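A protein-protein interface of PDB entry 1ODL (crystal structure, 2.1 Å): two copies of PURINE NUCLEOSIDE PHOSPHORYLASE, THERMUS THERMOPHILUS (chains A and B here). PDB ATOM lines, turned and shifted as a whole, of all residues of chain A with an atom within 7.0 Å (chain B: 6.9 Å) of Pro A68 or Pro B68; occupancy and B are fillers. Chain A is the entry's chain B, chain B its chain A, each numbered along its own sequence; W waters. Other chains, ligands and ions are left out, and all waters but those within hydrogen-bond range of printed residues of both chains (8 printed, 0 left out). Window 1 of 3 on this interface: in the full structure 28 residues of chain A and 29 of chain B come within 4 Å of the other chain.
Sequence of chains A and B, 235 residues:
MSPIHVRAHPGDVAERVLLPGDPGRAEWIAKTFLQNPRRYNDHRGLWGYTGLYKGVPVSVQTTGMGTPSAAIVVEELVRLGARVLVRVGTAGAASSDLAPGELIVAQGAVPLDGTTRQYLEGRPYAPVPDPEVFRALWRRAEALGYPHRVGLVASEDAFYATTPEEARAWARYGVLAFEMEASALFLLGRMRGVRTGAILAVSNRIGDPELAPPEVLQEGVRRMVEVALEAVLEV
Pro A68 touches Asp B157 (CB to O, 3.2 Å).
Met B65 touches Ser A69.
Gly A114 touches Gly B114 (CA to CA, 3.9 Å).
Gly A114 touches Asp B157.
Thr A115 touches Asp B157.
Pro B68 touches Asp A157.
OD1 of Asp A157 touches CA of Gly B114 (3.1 Å).
Asp A157 touches Asp B157.
Ile B72 touches Phe A159.
Met A180 touches Pro B68.
Pro A68 touches Met B180, and with the chains exchanged Met A180 touches Pro B68.
Ile A72 touches Phe B159, and with the chains exchanged Phe A159 touches Ile B72.
Gly B114 touches its own counterpart, Gly A114.
Thr A115 touches Asp B157, and with the chains exchanged Asp A157 touches Thr B115.
Positions printed for both chains: 63, 65, 66, 67, 68, 69, 70, 71, 72, 73, 113, 114, 115, 156, 157, 158, 159, 180 and 184.
Of the 19 pairs that touch across the chains among the printed residues, 17 have their exchanged pair printed and touching as well.
The backbone NH of Gly B66 sits close to the backbone carbonyl oxygen of Met B180, at 3.4 Å.
The side-chain hydroxyl (OG1) of Thr B67 is in hydrogen-bond range of the side-chain hydroxyl (OG1) of Thr B115.
The backbone carbonyl oxygen (O) of Thr A63 is in hydrogen-bond range of the side-chain hydroxyl (OG) of Ser A69 (2.6 Å).
OG1 of Thr A67 sits at hydrogen-bond distance from OG1 of Thr A115, 2.8 Å away.
The side-chain carboxylate (OD1) of Asp A113 is in hydrogen-bond range of the backbone NH (N) of Thr A115 (3.4 Å).
The side-chain carboxylate (OD1) of Asp A157 lies within hydrogen-bond range of the backbone NH (N) of Gly A114 (2.7 Å).
Printed residues of chain A that touch a printed residue of chain B: Met A65, Pro A68, Ser A69, Ile A72, Gly A114, Thr A115, Tyr A119, Asp A157, Phe A159 and Met A180.
Hydrophobic or aromatic side chains of chain A that line the printed part of chain B: Met A65, Pro A68, Ile A72, Tyr A119, Phe A159 and Met A180.
Of the 19 printed residues of chain B, 11 touch a printed residue of chain A.
Hydrophobic or aromatic side chains of chain B within 4 Å of the printed part of chain A: Pro B68, Ile B72, Ala B158, Phe B159 and Met B180.
Water W2 lies within hydrogen-bond range of O of Asp A157, O of Pro B68 and N of Phe A159.
Water W8 lies within hydrogen-bond range of OD1 of Asp B157 (2.7 Å), OD1 of Asp A157 (2.8 Å), N of Thr B115 (2.9 Å), OG1 of Thr B67 (2.9 Å) and N of Gly B114 (3.0 Å).
Water W6 lies within hydrogen-bond range of the backbone carbonyl oxygen of Pro A68 (2.7 Å), the backbone carbonyl oxygen of Asp B157 (2.9 Å) and the backbone NH of Phe B159 (3.0 Å).
Water W7 bridges the side-chain hydroxyl of Ser B69 and the backbone NH of Met A65.
Water W4 bridges OG of Ser A69 (2.8 Å) and N of Met B65 (2.8 Å).
Water W5 lies within hydrogen-bond range of OH of Tyr A119 (2.8 Å) and N of Phe B159 (3.1 Å).
Pro A68 touches four residues of chain B.
Printed residues of chain B within 4 Å of Ser A69: Met B65.
Of the printed residues of chain B, Ile A72 touches Phe B159 (3.6 Å) and Met B180 (3.8 Å).
Printed residues of chain B within 4 Å of Gly A114: Gly B114 (3.9 Å) and Asp B157 (3.1 Å).
Of the printed residues of chain B, Asp A157 touches Pro B68 (3.2 Å), Gly B114 (3.1 Å), Thr B115 (3.4 Å) and Asp B157 (3.6 Å).
Glu A181 touches none of the printed residues of chain B.
Of the printed residues of chain A, Ser B69 touches Met A65 (3.4 Å).
Val B73 touches none of the printed residues of chain A.
The nearest residue of chain B that does not touch Pro A68 is Met B65 (4.7 Å).
The side-chain carboxylate (OD1) of Asp A157 sits at hydrogen-bond distance from the backbone NH (N) of Thr B115, at 3.4 Å.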
ATOM      1  N   THR A  63      35.947  22.464 -20.407  1.00  0.00           N
ATOM      2  CA  THR A  63      34.854  22.122 -19.493  1.00  0.00           C
ATOM      3  C   THR A  63      34.424  20.662 -19.606  1.00  0.00           C
ATOM      4  O   THR A  63      33.774  20.133 -18.707  1.00  0.00           O
ATOM      5  CB  THR A  63      33.588  22.961 -19.763  1.00  0.00           C
ATOM      6  OG1 THR A  63      33.088  22.651 -21.070  1.00  0.00           O
ATOM      7  CG2 THR A  63      33.886  24.469 -19.665  1.00  0.00           C
ATOM      8  N   MET A  65      32.314  17.657 -21.802  1.00  0.00           N
ATOM      9  CA  MET A  65      30.979  17.689 -22.388  1.00  0.00           C
ATOM     10  C   MET A  65      29.905  17.429 -21.346  1.00  0.00           C
ATOM     11  O   MET A  65      30.037  16.515 -20.531  1.00  0.00           O
ATOM     12  CB  MET A  65      30.849  16.631 -23.482  1.00  0.00           C
ATOM     13  CG  MET A  65      31.759  16.825 -24.681  1.00  0.00           C
ATOM     14  SD  MET A  65      31.520  15.499 -25.888  1.00  0.00           S
ATOM     15  CE  MET A  65      32.368  14.117 -25.041  1.00  0.00           C
ATOM     16  N   GLY A  66      28.840  18.225 -21.388  1.00  0.00           N
ATOM     17  CA  GLY A  66      27.734  18.047 -20.458  1.00  0.00           C
ATOM     18  C   GLY A  66      27.739  19.009 -19.290  1.00  0.00           C
ATOM     19  O   GLY A  66      28.796  19.458 -18.859  1.00  0.00           O
ATOM     20  N   THR A  67      26.556  19.322 -18.765  1.00  0.00           N
ATOM     21  CA  THR A  67      26.456  20.243 -17.640  1.00  0.00           C
ATOM     22  C   THR A  67      27.087  19.732 -16.346  1.00  0.00           C
ATOM     23  O   THR A  67      27.584  20.526 -15.540  1.00  0.00           O
ATOM     24  CB  THR A  67      24.985  20.650 -17.368  1.00  0.00           C
ATOM     25  OG1 THR A  67      24.161  19.480 -17.274  1.00  0.00           O
ATOM     26  CG2 THR A  67      24.466  21.543 -18.491  1.00  0.00           C
ATOM     27  N   PRO A  68      27.087  18.406 -16.120  1.00  0.00           N
ATOM     28  CA  PRO A  68      27.704  17.951 -14.868  1.00  0.00           C
ATOM     29  C   PRO A  68      29.189  18.283 -14.880  1.00  0.00           C
ATOM     30  O   PRO A  68      29.735  18.799 -13.907  1.00  0.00           O
ATOM     31  CB  PRO A  68      27.450  16.443 -14.877  1.00  0.00           C
ATOM     32  CG  PRO A  68      26.170  16.321 -15.671  1.00  0.00           C
ATOM     33  CD  PRO A  68      26.410  17.291 -16.807  1.00  0.00           C
ATOM     34  N   SER A  69      29.829  17.992 -16.006  1.00  0.00           N
ATOM     35  CA  SER A  69      31.246  18.253 -16.165  1.00  0.00           C
ATOM     36  C   SER A  69      31.521  19.751 -16.127  1.00  0.00           C
ATOM     37  O   SER A  69      32.437  20.202 -15.441  1.00  0.00           O
ATOM     38  CB  SER A  69      31.735  17.666 -17.490  1.00  0.00           C
ATOM     39  OG  SER A  69      33.131  17.828 -17.632  1.00  0.00           O
ATOM     40  N   ALA A  70      30.719  20.524 -16.854  1.00  0.00           N
ATOM     41  CA  ALA A  70      30.908  21.968 -16.895  1.00  0.00           C
ATOM     42  C   ALA A  70      30.645  22.650 -15.554  1.00  0.00           C
ATOM     43  O   ALA A  70      31.280  23.656 -15.234  1.00  0.00           O
ATOM     44  CB  ALA A  70      30.023  22.582 -17.977  1.00  0.00           C
ATOM     45  N   ALA A  71      29.707  22.122 -14.774  1.00  0.00           N
ATOM     46  CA  ALA A  71      29.392  22.728 -13.479  1.00  0.00           C
ATOM     47  C   ALA A  71      30.575  22.560 -12.535  1.00  0.00           C
ATOM     48  O   ALA A  71      30.908  23.457 -11.770  1.00  0.00           O
ATOM     49  CB  ALA A  71      28.147  22.089 -12.877  1.00  0.00           C
ATOM     50  N   ILE A  72      31.204  21.394 -12.597  1.00  0.00           N
ATOM     51  CA  ILE A  72      32.357  21.109 -11.761  1.00  0.00           C
ATOM     52  C   ILE A  72      33.475  22.105 -12.057  1.00  0.00           C
ATOM     53  O   ILE A  72      34.082  22.656 -11.137  1.00  0.00           O
ATOM     54  CB  ILE A  72      32.854  19.669 -12.014  1.00  0.00           C
ATOM     55  CG1 ILE A  72      31.923  18.680 -11.303  1.00  0.00           C
ATOM     56  CG2 ILE A  72      34.306  19.520 -11.582  1.00  0.00           C
ATOM     57  CD1 ILE A  72      32.254  17.215 -11.569  1.00  0.00           C
ATOM     58  N   VAL A  73      33.731  22.341 -13.342  1.00  0.00           N
ATOM     59  CA  VAL A  73      34.777  23.267 -13.771  1.00  0.00           C
ATOM     60  C   VAL A  73      34.453  24.712 -13.417  1.00  0.00           C
ATOM     61  O   VAL A  73      35.315  25.448 -12.934  1.00  0.00           O
ATOM     62  CB  VAL A  73      35.021  23.171 -15.301  1.00  0.00           C
ATOM     63  CG1 VAL A  73      35.995  24.256 -15.750  1.00  0.00           C
ATOM     64  CG2 VAL A  73      35.586  21.804 -15.650  1.00  0.00           C
ATOM     65  N   ASP A 113      18.478  19.747 -18.924  1.00  0.00           N
ATOM     66  CA  ASP A 113      19.510  18.964 -18.237  1.00  0.00           C
ATOM     67  C   ASP A 113      19.201  18.739 -16.753  1.00  0.00           C
ATOM     68  O   ASP A 113      18.409  19.473 -16.156  1.00  0.00           O
ATOM     69  CB  ASP A 113      20.858  19.668 -18.346  1.00  0.00           C
ATOM     70  CG  ASP A 113      20.911  20.945 -17.521  1.00  0.00           C
ATOM     71  OD1 ASP A 113      21.857  21.101 -16.718  1.00  0.00           O
ATOM     72  OD2 ASP A 113      19.999  21.786 -17.672  1.00  0.00           O
ATOM     73  N   GLY A 114      19.854  17.742 -16.155  1.00  0.00           N
ATOM     74  CA  GLY A 114      19.624  17.433 -14.750  1.00  0.00           C
ATOM     75  C   GLY A 114      20.525  18.159 -13.760  1.00  0.00           C
ATOM     76  O   GLY A 114      20.297  18.103 -12.550  1.00  0.00           O
ATOM     77  N   THR A 115      21.558  18.834 -14.250  1.00  0.00           N
ATOM     78  CA  THR A 115      22.450  19.556 -13.348  1.00  0.00           C
ATOM     79  C   THR A 115      21.735  20.786 -12.787  1.00  0.00           C
ATOM     80  O   THR A 115      21.698  20.984 -11.572  1.00  0.00           O
ATOM     81  CB  THR A 115      23.750  19.993 -14.060  1.00  0.00           C
ATOM     82  OG1 THR A 115      24.399  18.837 -14.602  1.00  0.00           O
ATOM     83  CG2 THR A 115      24.694  20.684 -13.076  1.00  0.00           C
ATOM     84  N   TYR A 119      20.501  21.502  -8.780  1.00  0.00           N
ATOM     85  CA  TYR A 119      20.799  22.749  -8.078  1.00  0.00           C
ATOM     86  C   TYR A 119      19.515  23.472  -7.681  1.00  0.00           C
ATOM     87  O   TYR A 119      19.437  24.076  -6.611  1.00  0.00           O
ATOM     88  CB  TYR A 119      21.610  23.699  -8.964  1.00  0.00           C
ATOM     89  CG  TYR A 119      23.102  23.464  -8.971  1.00  0.00           C
ATOM     90  CD1 TYR A 119      23.748  22.998 -10.114  1.00  0.00           C
ATOM     91  CD2 TYR A 119      23.875  23.742  -7.844  1.00  0.00           C
ATOM     92  CE1 TYR A 119      25.131  22.821 -10.137  1.00  0.00           C
ATOM     93  CE2 TYR A 119      25.260  23.570  -7.857  1.00  0.00           C
ATOM     94  CZ  TYR A 119      25.881  23.112  -9.004  1.00  0.00           C
ATOM     95  OH  TYR A 119      27.252  22.971  -9.027  1.00  0.00           O
ATOM     96  N   GLU A 156      20.845  20.133 -23.339  1.00  0.00           N
ATOM     97  CA  GLU A 156      20.354  18.777 -23.117  1.00  0.00           C
ATOM     98  C   GLU A 156      21.415  17.849 -22.515  1.00  0.00           C
ATOM     99  O   GLU A 156      22.605  18.174 -22.509  1.00  0.00           O
ATOM    100  CB  GLU A 156      19.860  18.199 -24.444  1.00  0.00           C
ATOM    101  CG  GLU A 156      20.912  18.251 -25.539  1.00  0.00           C
ATOM    102  CD  GLU A 156      20.488  17.522 -26.784  1.00  0.00           C
ATOM    103  OE1 GLU A 156      21.259  17.515 -27.764  1.00  0.00           O
ATOM    104  OE2 GLU A 156      19.382  16.949 -26.782  1.00  0.00           O
ATOM    105  N   ASP A 157      20.970  16.699 -22.011  1.00  0.00           N
ATOM    106  CA  ASP A 157      21.857  15.700 -21.410  1.00  0.00           C
ATOM    107  C   ASP A 157      22.095  14.506 -22.330  1.00  0.00           C
ATOM    108  O   ASP A 157      23.210  13.998 -22.412  1.00  0.00           O
ATOM    109  CB  ASP A 157      21.265  15.183 -20.095  1.00  0.00           C
ATOM    110  CG  ASP A 157      21.483  16.135 -18.933  1.00  0.00           C
ATOM    111  OD1 ASP A 157      20.838  15.921 -17.886  1.00  0.00           O
ATOM    112  OD2 ASP A 157      22.300  17.081 -19.056  1.00  0.00           O
ATOM    113  N   ALA A 158      21.039  14.052 -23.002  1.00  0.00           N
ATOM    114  CA  ALA A 158      21.121  12.898 -23.899  1.00  0.00           C
ATOM    115  C   ALA A 158      21.252  13.301 -25.366  1.00  0.00           C
ATOM    116  O   ALA A 158      20.256  13.446 -26.085  1.00  0.00           O
ATOM    117  CB  ALA A 158      19.905  12.009 -23.710  1.00  0.00           C
ATOM    118  N   PHE A 159      22.499  13.465 -25.790  1.00  0.00           N
ATOM    119  CA  PHE A 159      22.852  13.857 -27.147  1.00  0.00           C
ATOM    120  C   PHE A 159      22.187  12.988 -28.211  1.00  0.00           C
ATOM    121  O   PHE A 159      21.651  13.505 -29.189  1.00  0.00           O
ATOM    122  CB  PHE A 159      24.377  13.791 -27.295  1.00  0.00           C
ATOM    123  CG  PHE A 159      24.890  14.252 -28.625  1.00  0.00           C
ATOM    124  CD1 PHE A 159      25.173  15.596 -28.853  1.00  0.00           C
ATOM    125  CD2 PHE A 159      25.109  13.336 -29.653  1.00  0.00           C
ATOM    126  CE1 PHE A 159      25.672  16.023 -30.094  1.00  0.00           C
ATOM    127  CE2 PHE A 159      25.606  13.754 -30.892  1.00  0.00           C
ATOM    128  CZ  PHE A 159      25.888  15.094 -31.112  1.00  0.00           C
ATOM    129  N   MET A 180      25.190  21.405 -24.869  1.00  0.00           N
ATOM    130  CA  MET A 180      25.152  20.694 -23.593  1.00  0.00           C
ATOM    131  C   MET A 180      25.849  21.332 -22.400  1.00  0.00           C
ATOM    132  O   MET A 180      26.403  20.609 -21.563  1.00  0.00           O
ATOM    133  CB  MET A 180      25.735  19.291 -23.804  1.00  0.00           C
ATOM    134  CG  MET A 180      25.080  18.506 -24.934  1.00  0.00           C
ATOM    135  SD  MET A 180      25.952  16.973 -25.299  1.00  0.00           S
ATOM    136  CE  MET A 180      25.567  16.037 -23.839  1.00  0.00           C
ATOM    137  N   GLU A 181      25.823  22.659 -22.287  1.00  0.00           N
ATOM    138  CA  GLU A 181      26.516  23.290 -21.164  1.00  0.00           C
ATOM    139  C   GLU A 181      25.971  24.624 -20.670  1.00  0.00           C
ATOM    140  O   GLU A 181      26.061  24.930 -19.482  1.00  0.00           O
ATOM    141  CB  GLU A 181      27.998  23.480 -21.504  1.00  0.00           C
ATOM    142  CG  GLU A 181      28.812  22.196 -21.665  1.00  0.00           C
ATOM    143  CD  GLU A 181      28.778  21.625 -23.076  1.00  0.00           C
ATOM    144  OE1 GLU A 181      29.422  20.579 -23.300  1.00  0.00           O
ATOM    145  OE2 GLU A 181      28.120  22.215 -23.961  1.00  0.00           O
ATOM    146  N   ALA A 184      23.644  25.382 -17.130  1.00  0.00           N
ATOM    147  CA  ALA A 184      24.323  25.323 -15.838  1.00  0.00           C
ATOM    148  C   ALA A 184      25.287  26.498 -15.627  1.00  0.00           C
ATOM    149  O   ALA A 184      25.460  26.966 -14.503  1.00  0.00           O
ATOM    150  CB  ALA A 184      25.072  23.993 -15.699  1.00  0.00           C
ATOM    151  N   THR B  63      35.505   8.063 -20.485  1.00  0.00           N
ATOM    152  CA  THR B  63      34.115   8.491 -20.639  1.00  0.00           C
ATOM    153  C   THR B  63      33.918   9.964 -20.328  1.00  0.00           C
ATOM    154  O   THR B  63      32.960  10.574 -20.793  1.00  0.00           O
ATOM    155  CB  THR B  63      33.150   7.720 -19.704  1.00  0.00           C
ATOM    156  OG1 THR B  63      33.554   7.920 -18.344  1.00  0.00           O
ATOM    157  CG2 THR B  63      33.138   6.216 -20.027  1.00  0.00           C
ATOM    158  N   MET B  65      33.514  13.016 -17.293  1.00  0.00           N
ATOM    159  CA  MET B  65      32.665  13.056 -16.103  1.00  0.00           C
ATOM    160  C   MET B  65      31.207  13.394 -16.419  1.00  0.00           C
ATOM    161  O   MET B  65      30.935  14.289 -17.211  1.00  0.00           O
ATOM    162  CB  MET B  65      33.200  14.089 -15.109  1.00  0.00           C
ATOM    163  CG  MET B  65      34.598  13.795 -14.586  1.00  0.00           C
ATOM    164  SD  MET B  65      35.149  15.029 -13.389  1.00  0.00           S
ATOM    165  CE  MET B  65      35.413  16.424 -14.456  1.00  0.00           C
ATOM    166  N   GLY B  66      30.278  12.681 -15.787  1.00  0.00           N
ATOM    167  CA  GLY B  66      28.867  12.939 -16.007  1.00  0.00           C
ATOM    168  C   GLY B  66      28.235  11.983 -16.997  1.00  0.00           C
ATOM    169  O   GLY B  66      28.887  11.548 -17.955  1.00  0.00           O
ATOM    170  N   THR B  67      26.966  11.660 -16.768  1.00  0.00           N
ATOM    171  CA  THR B  67      26.232  10.743 -17.640  1.00  0.00           C
ATOM    172  C   THR B  67      26.077  11.250 -19.067  1.00  0.00           C
ATOM    173  O   THR B  67      26.041  10.451 -20.006  1.00  0.00           O
ATOM    174  CB  THR B  67      24.828  10.408 -17.069  1.00  0.00           C
ATOM    175  OG1 THR B  67      24.160  11.615 -16.674  1.00  0.00           O
ATOM    176  CG2 THR B  67      24.958   9.471 -15.864  1.00  0.00           C
ATOM    177  N   PRO B  68      25.969  12.581 -19.255  1.00  0.00           N
ATOM    178  CA  PRO B  68      25.826  13.096 -20.622  1.00  0.00           C
ATOM    179  C   PRO B  68      27.057  12.749 -21.452  1.00  0.00           C
ATOM    180  O   PRO B  68      26.953  12.366 -22.617  1.00  0.00           O
ATOM    181  CB  PRO B  68      25.673  14.603 -20.408  1.00  0.00           C
ATOM    182  CG  PRO B  68      24.980  14.679 -19.081  1.00  0.00           C
ATOM    183  CD  PRO B  68      25.742  13.653 -18.270  1.00  0.00           C
ATOM    184  N   SER B  69      28.227  12.890 -20.834  1.00  0.00           N
ATOM    185  CA  SER B  69      29.494  12.591 -21.490  1.00  0.00           C
ATOM    186  C   SER B  69      29.659  11.077 -21.654  1.00  0.00           C
ATOM    187  O   SER B  69      30.063  10.598 -22.703  1.00  0.00           O
ATOM    188  CB  SER B  69      30.658  13.154 -20.658  1.00  0.00           C
ATOM    189  OG  SER B  69      31.904  12.948 -21.304  1.00  0.00           O
ATOM    190  N   ALA B  70      29.340  10.331 -20.603  1.00  0.00           N
ATOM    191  CA  ALA B  70      29.458   8.875 -20.629  1.00  0.00           C
ATOM    192  C   ALA B  70      28.482   8.248 -21.626  1.00  0.00           C
ATOM    193  O   ALA B  70      28.829   7.287 -22.309  1.00  0.00           O
ATOM    194  CB  ALA B  70      29.218   8.316 -19.239  1.00  0.00           C
ATOM    195  N   ALA B  71      27.269   8.799 -21.705  1.00  0.00           N
ATOM    196  CA  ALA B  71      26.240   8.307 -22.616  1.00  0.00           C
ATOM    197  C   ALA B  71      26.694   8.457 -24.063  1.00  0.00           C
ATOM    198  O   ALA B  71      26.470   7.575 -24.890  1.00  0.00           O
ATOM    199  CB  ALA B  71      24.942   9.066 -22.392  1.00  0.00           C
ATOM    200  N   ILE B  72      27.328   9.585 -24.366  1.00  0.00           N
ATOM    201  CA  ILE B  72      27.839   9.828 -25.709  1.00  0.00           C
ATOM    202  C   ILE B  72      28.890   8.773 -26.030  1.00  0.00           C
ATOM    203  O   ILE B  72      28.850   8.136 -27.083  1.00  0.00           O
ATOM    204  CB  ILE B  72      28.486  11.234 -25.825  1.00  0.00           C
ATOM    205  CG1 ILE B  72      27.396  12.280 -26.039  1.00  0.00           C
ATOM    206  CG2 ILE B  72      29.505  11.266 -26.973  1.00  0.00           C
ATOM    207  CD1 ILE B  72      27.883  13.713 -25.948  1.00  0.00           C
ATOM    208  N   VAL B  73      29.824   8.577 -25.109  1.00  0.00           N
ATOM    209  CA  VAL B  73      30.880   7.604 -25.331  1.00  0.00           C
ATOM    210  C   VAL B  73      30.329   6.180 -25.463  1.00  0.00           C
ATOM    211  O   VAL B  73      30.701   5.452 -26.384  1.00  0.00           O
ATOM    212  CB  VAL B  73      31.935   7.673 -24.202  1.00  0.00           C
ATOM    213  CG1 VAL B  73      32.976   6.584 -24.393  1.00  0.00           C
ATOM    214  CG2 VAL B  73      32.607   9.044 -24.208  1.00  0.00           C
ATOM    215  N   ASP B 113      20.241  11.517 -12.270  1.00  0.00           N
ATOM    216  CA  ASP B 113      20.757  12.292 -13.391  1.00  0.00           C
ATOM    217  C   ASP B 113      19.710  12.572 -14.469  1.00  0.00           C
ATOM    218  O   ASP B 113      18.704  11.878 -14.565  1.00  0.00           O
ATOM    219  CB  ASP B 113      21.940  11.562 -14.020  1.00  0.00           C
ATOM    220  CG  ASP B 113      21.519  10.291 -14.729  1.00  0.00           C
ATOM    221  OD1 ASP B 113      21.800  10.179 -15.935  1.00  0.00           O
ATOM    222  OD2 ASP B 113      20.897   9.414 -14.084  1.00  0.00           O
ATOM    223  N   GLY B 114      19.964  13.596 -15.277  1.00  0.00           N
ATOM    224  CA  GLY B 114      19.045  13.968 -16.341  1.00  0.00           C
ATOM    225  C   GLY B 114      19.196  13.181 -17.631  1.00  0.00           C
ATOM    226  O   GLY B 114      18.265  13.128 -18.432  1.00  0.00           O
ATOM    227  N   THR B 115      20.353  12.564 -17.848  1.00  0.00           N
ATOM    228  CA  THR B 115      20.559  11.790 -19.065  1.00  0.00           C
ATOM    229  C   THR B 115      19.563  10.632 -19.117  1.00  0.00           C
ATOM    230  O   THR B 115      18.834  10.470 -20.101  1.00  0.00           O
ATOM    231  CB  THR B 115      21.991  11.236 -19.143  1.00  0.00           C
ATOM    232  OG1 THR B 115      22.924  12.324 -19.114  1.00  0.00           O
ATOM    233  CG2 THR B 115      22.185  10.445 -20.433  1.00  0.00           C
ATOM    234  N   GLU B 156      24.725  11.036  -9.776  1.00  0.00           N
ATOM    235  CA  GLU B 156      24.275  12.429  -9.713  1.00  0.00           C
ATOM    236  C   GLU B 156      24.839  13.313 -10.831  1.00  0.00           C
ATOM    237  O   GLU B 156      25.825  12.969 -11.481  1.00  0.00           O
ATOM    238  CB  GLU B 156      24.698  13.032  -8.381  1.00  0.00           C
ATOM    239  CG  GLU B 156      26.210  13.017  -8.224  1.00  0.00           C
ATOM    240  CD  GLU B 156      26.685  13.663  -6.942  1.00  0.00           C
ATOM    241  OE1 GLU B 156      27.915  13.659  -6.700  1.00  0.00           O
ATOM    242  OE2 GLU B 156      25.836  14.172  -6.180  1.00  0.00           O
ATOM    243  N   ASP B 157      24.215  14.473 -11.012  1.00  0.00           N
ATOM    244  CA  ASP B 157      24.619  15.443 -12.016  1.00  0.00           C
ATOM    245  C   ASP B 157      25.355  16.626 -11.390  1.00  0.00           C
ATOM    246  O   ASP B 157      26.372  17.078 -11.912  1.00  0.00           O
ATOM    247  CB  ASP B 157      23.393  15.967 -12.767  1.00  0.00           C
ATOM    248  CG  ASP B 157      22.975  15.070 -13.911  1.00  0.00           C
ATOM    249  OD1 ASP B 157      21.895  15.316 -14.489  1.00  0.00           O
ATOM    250  OD2 ASP B 157      23.728  14.128 -14.243  1.00  0.00           O
ATOM    251  N   ALA B 158      24.836  17.131 -10.274  1.00  0.00           N
ATOM    252  CA  ALA B 158      25.448  18.284  -9.612  1.00  0.00           C
ATOM    253  C   ALA B 158      26.401  17.881  -8.487  1.00  0.00           C
ATOM    254  O   ALA B 158      26.006  17.787  -7.330  1.00  0.00           O
ATOM    255  CB  ALA B 158      24.357  19.218  -9.077  1.00  0.00           C
ATOM    256  N   PHE B 159      27.665  17.670  -8.845  1.00  0.00           N
ATOM    257  CA  PHE B 159      28.685  17.259  -7.887  1.00  0.00           C
ATOM    258  C   PHE B 159      28.709  18.162  -6.659  1.00  0.00           C
ATOM    259  O   PHE B 159      28.735  17.676  -5.530  1.00  0.00           O
ATOM    260  CB  PHE B 159      30.065  17.277  -8.550  1.00  0.00           C
ATOM    261  CG  PHE B 159      31.191  16.816  -7.648  1.00  0.00           C
ATOM    262  CD1 PHE B 159      31.499  15.461  -7.521  1.00  0.00           C
ATOM    263  CD2 PHE B 159      31.950  17.743  -6.935  1.00  0.00           C
ATOM    264  CE1 PHE B 159      32.553  15.035  -6.699  1.00  0.00           C
ATOM    265  CE2 PHE B 159      33.004  17.331  -6.111  1.00  0.00           C
ATOM    266  CZ  PHE B 159      33.307  15.973  -5.994  1.00  0.00           C
ATOM    267  N   MET B 180      29.099   9.604 -10.966  1.00  0.00           N
ATOM    268  CA  MET B 180      28.407  10.324 -12.030  1.00  0.00           C
ATOM    269  C   MET B 180      28.279   9.656 -13.397  1.00  0.00           C
ATOM    270  O   MET B 180      28.300  10.350 -14.416  1.00  0.00           O
ATOM    271  CB  MET B 180      29.104  11.676 -12.206  1.00  0.00           C
ATOM    272  CG  MET B 180      29.230  12.478 -10.910  1.00  0.00           C
ATOM    273  SD  MET B 180      30.188  14.011 -11.078  1.00  0.00           S
ATOM    274  CE  MET B 180      29.192  14.910 -12.263  1.00  0.00           C
ATOM    275  N   ALA B 184      23.367   5.786 -16.419  1.00  0.00           N
ATOM    276  CA  ALA B 184      23.261   5.840 -17.881  1.00  0.00           C
ATOM    277  C   ALA B 184      23.851   4.615 -18.570  1.00  0.00           C
ATOM    278  O   ALA B 184      23.328   4.148 -19.587  1.00  0.00           O
ATOM    279  CB  ALA B 184      23.930   7.114 -18.418  1.00  0.00           C
HETATM  280  O   HOH W   1      28.958  15.493 -18.300  1.00  0.00           O
HETATM  281  O   HOH W   2      24.387  12.389 -23.820  1.00  0.00           O
HETATM  282  O   HOH W   3      22.835  17.315 -16.463  1.00  0.00           O
HETATM  283  O   HOH W   4      34.347  15.451 -18.503  1.00  0.00           O
HETATM  284  O   HOH W   5      28.643  20.534  -9.410  1.00  0.00           O
HETATM  285  O   HOH W   6      28.593  18.914 -11.410  1.00  0.00           O
HETATM  286  O   HOH W   7      33.583  15.139 -21.262  1.00  0.00           O
HETATM  287  O   HOH W   8      22.567  14.020 -16.734  1.00  0.00           O
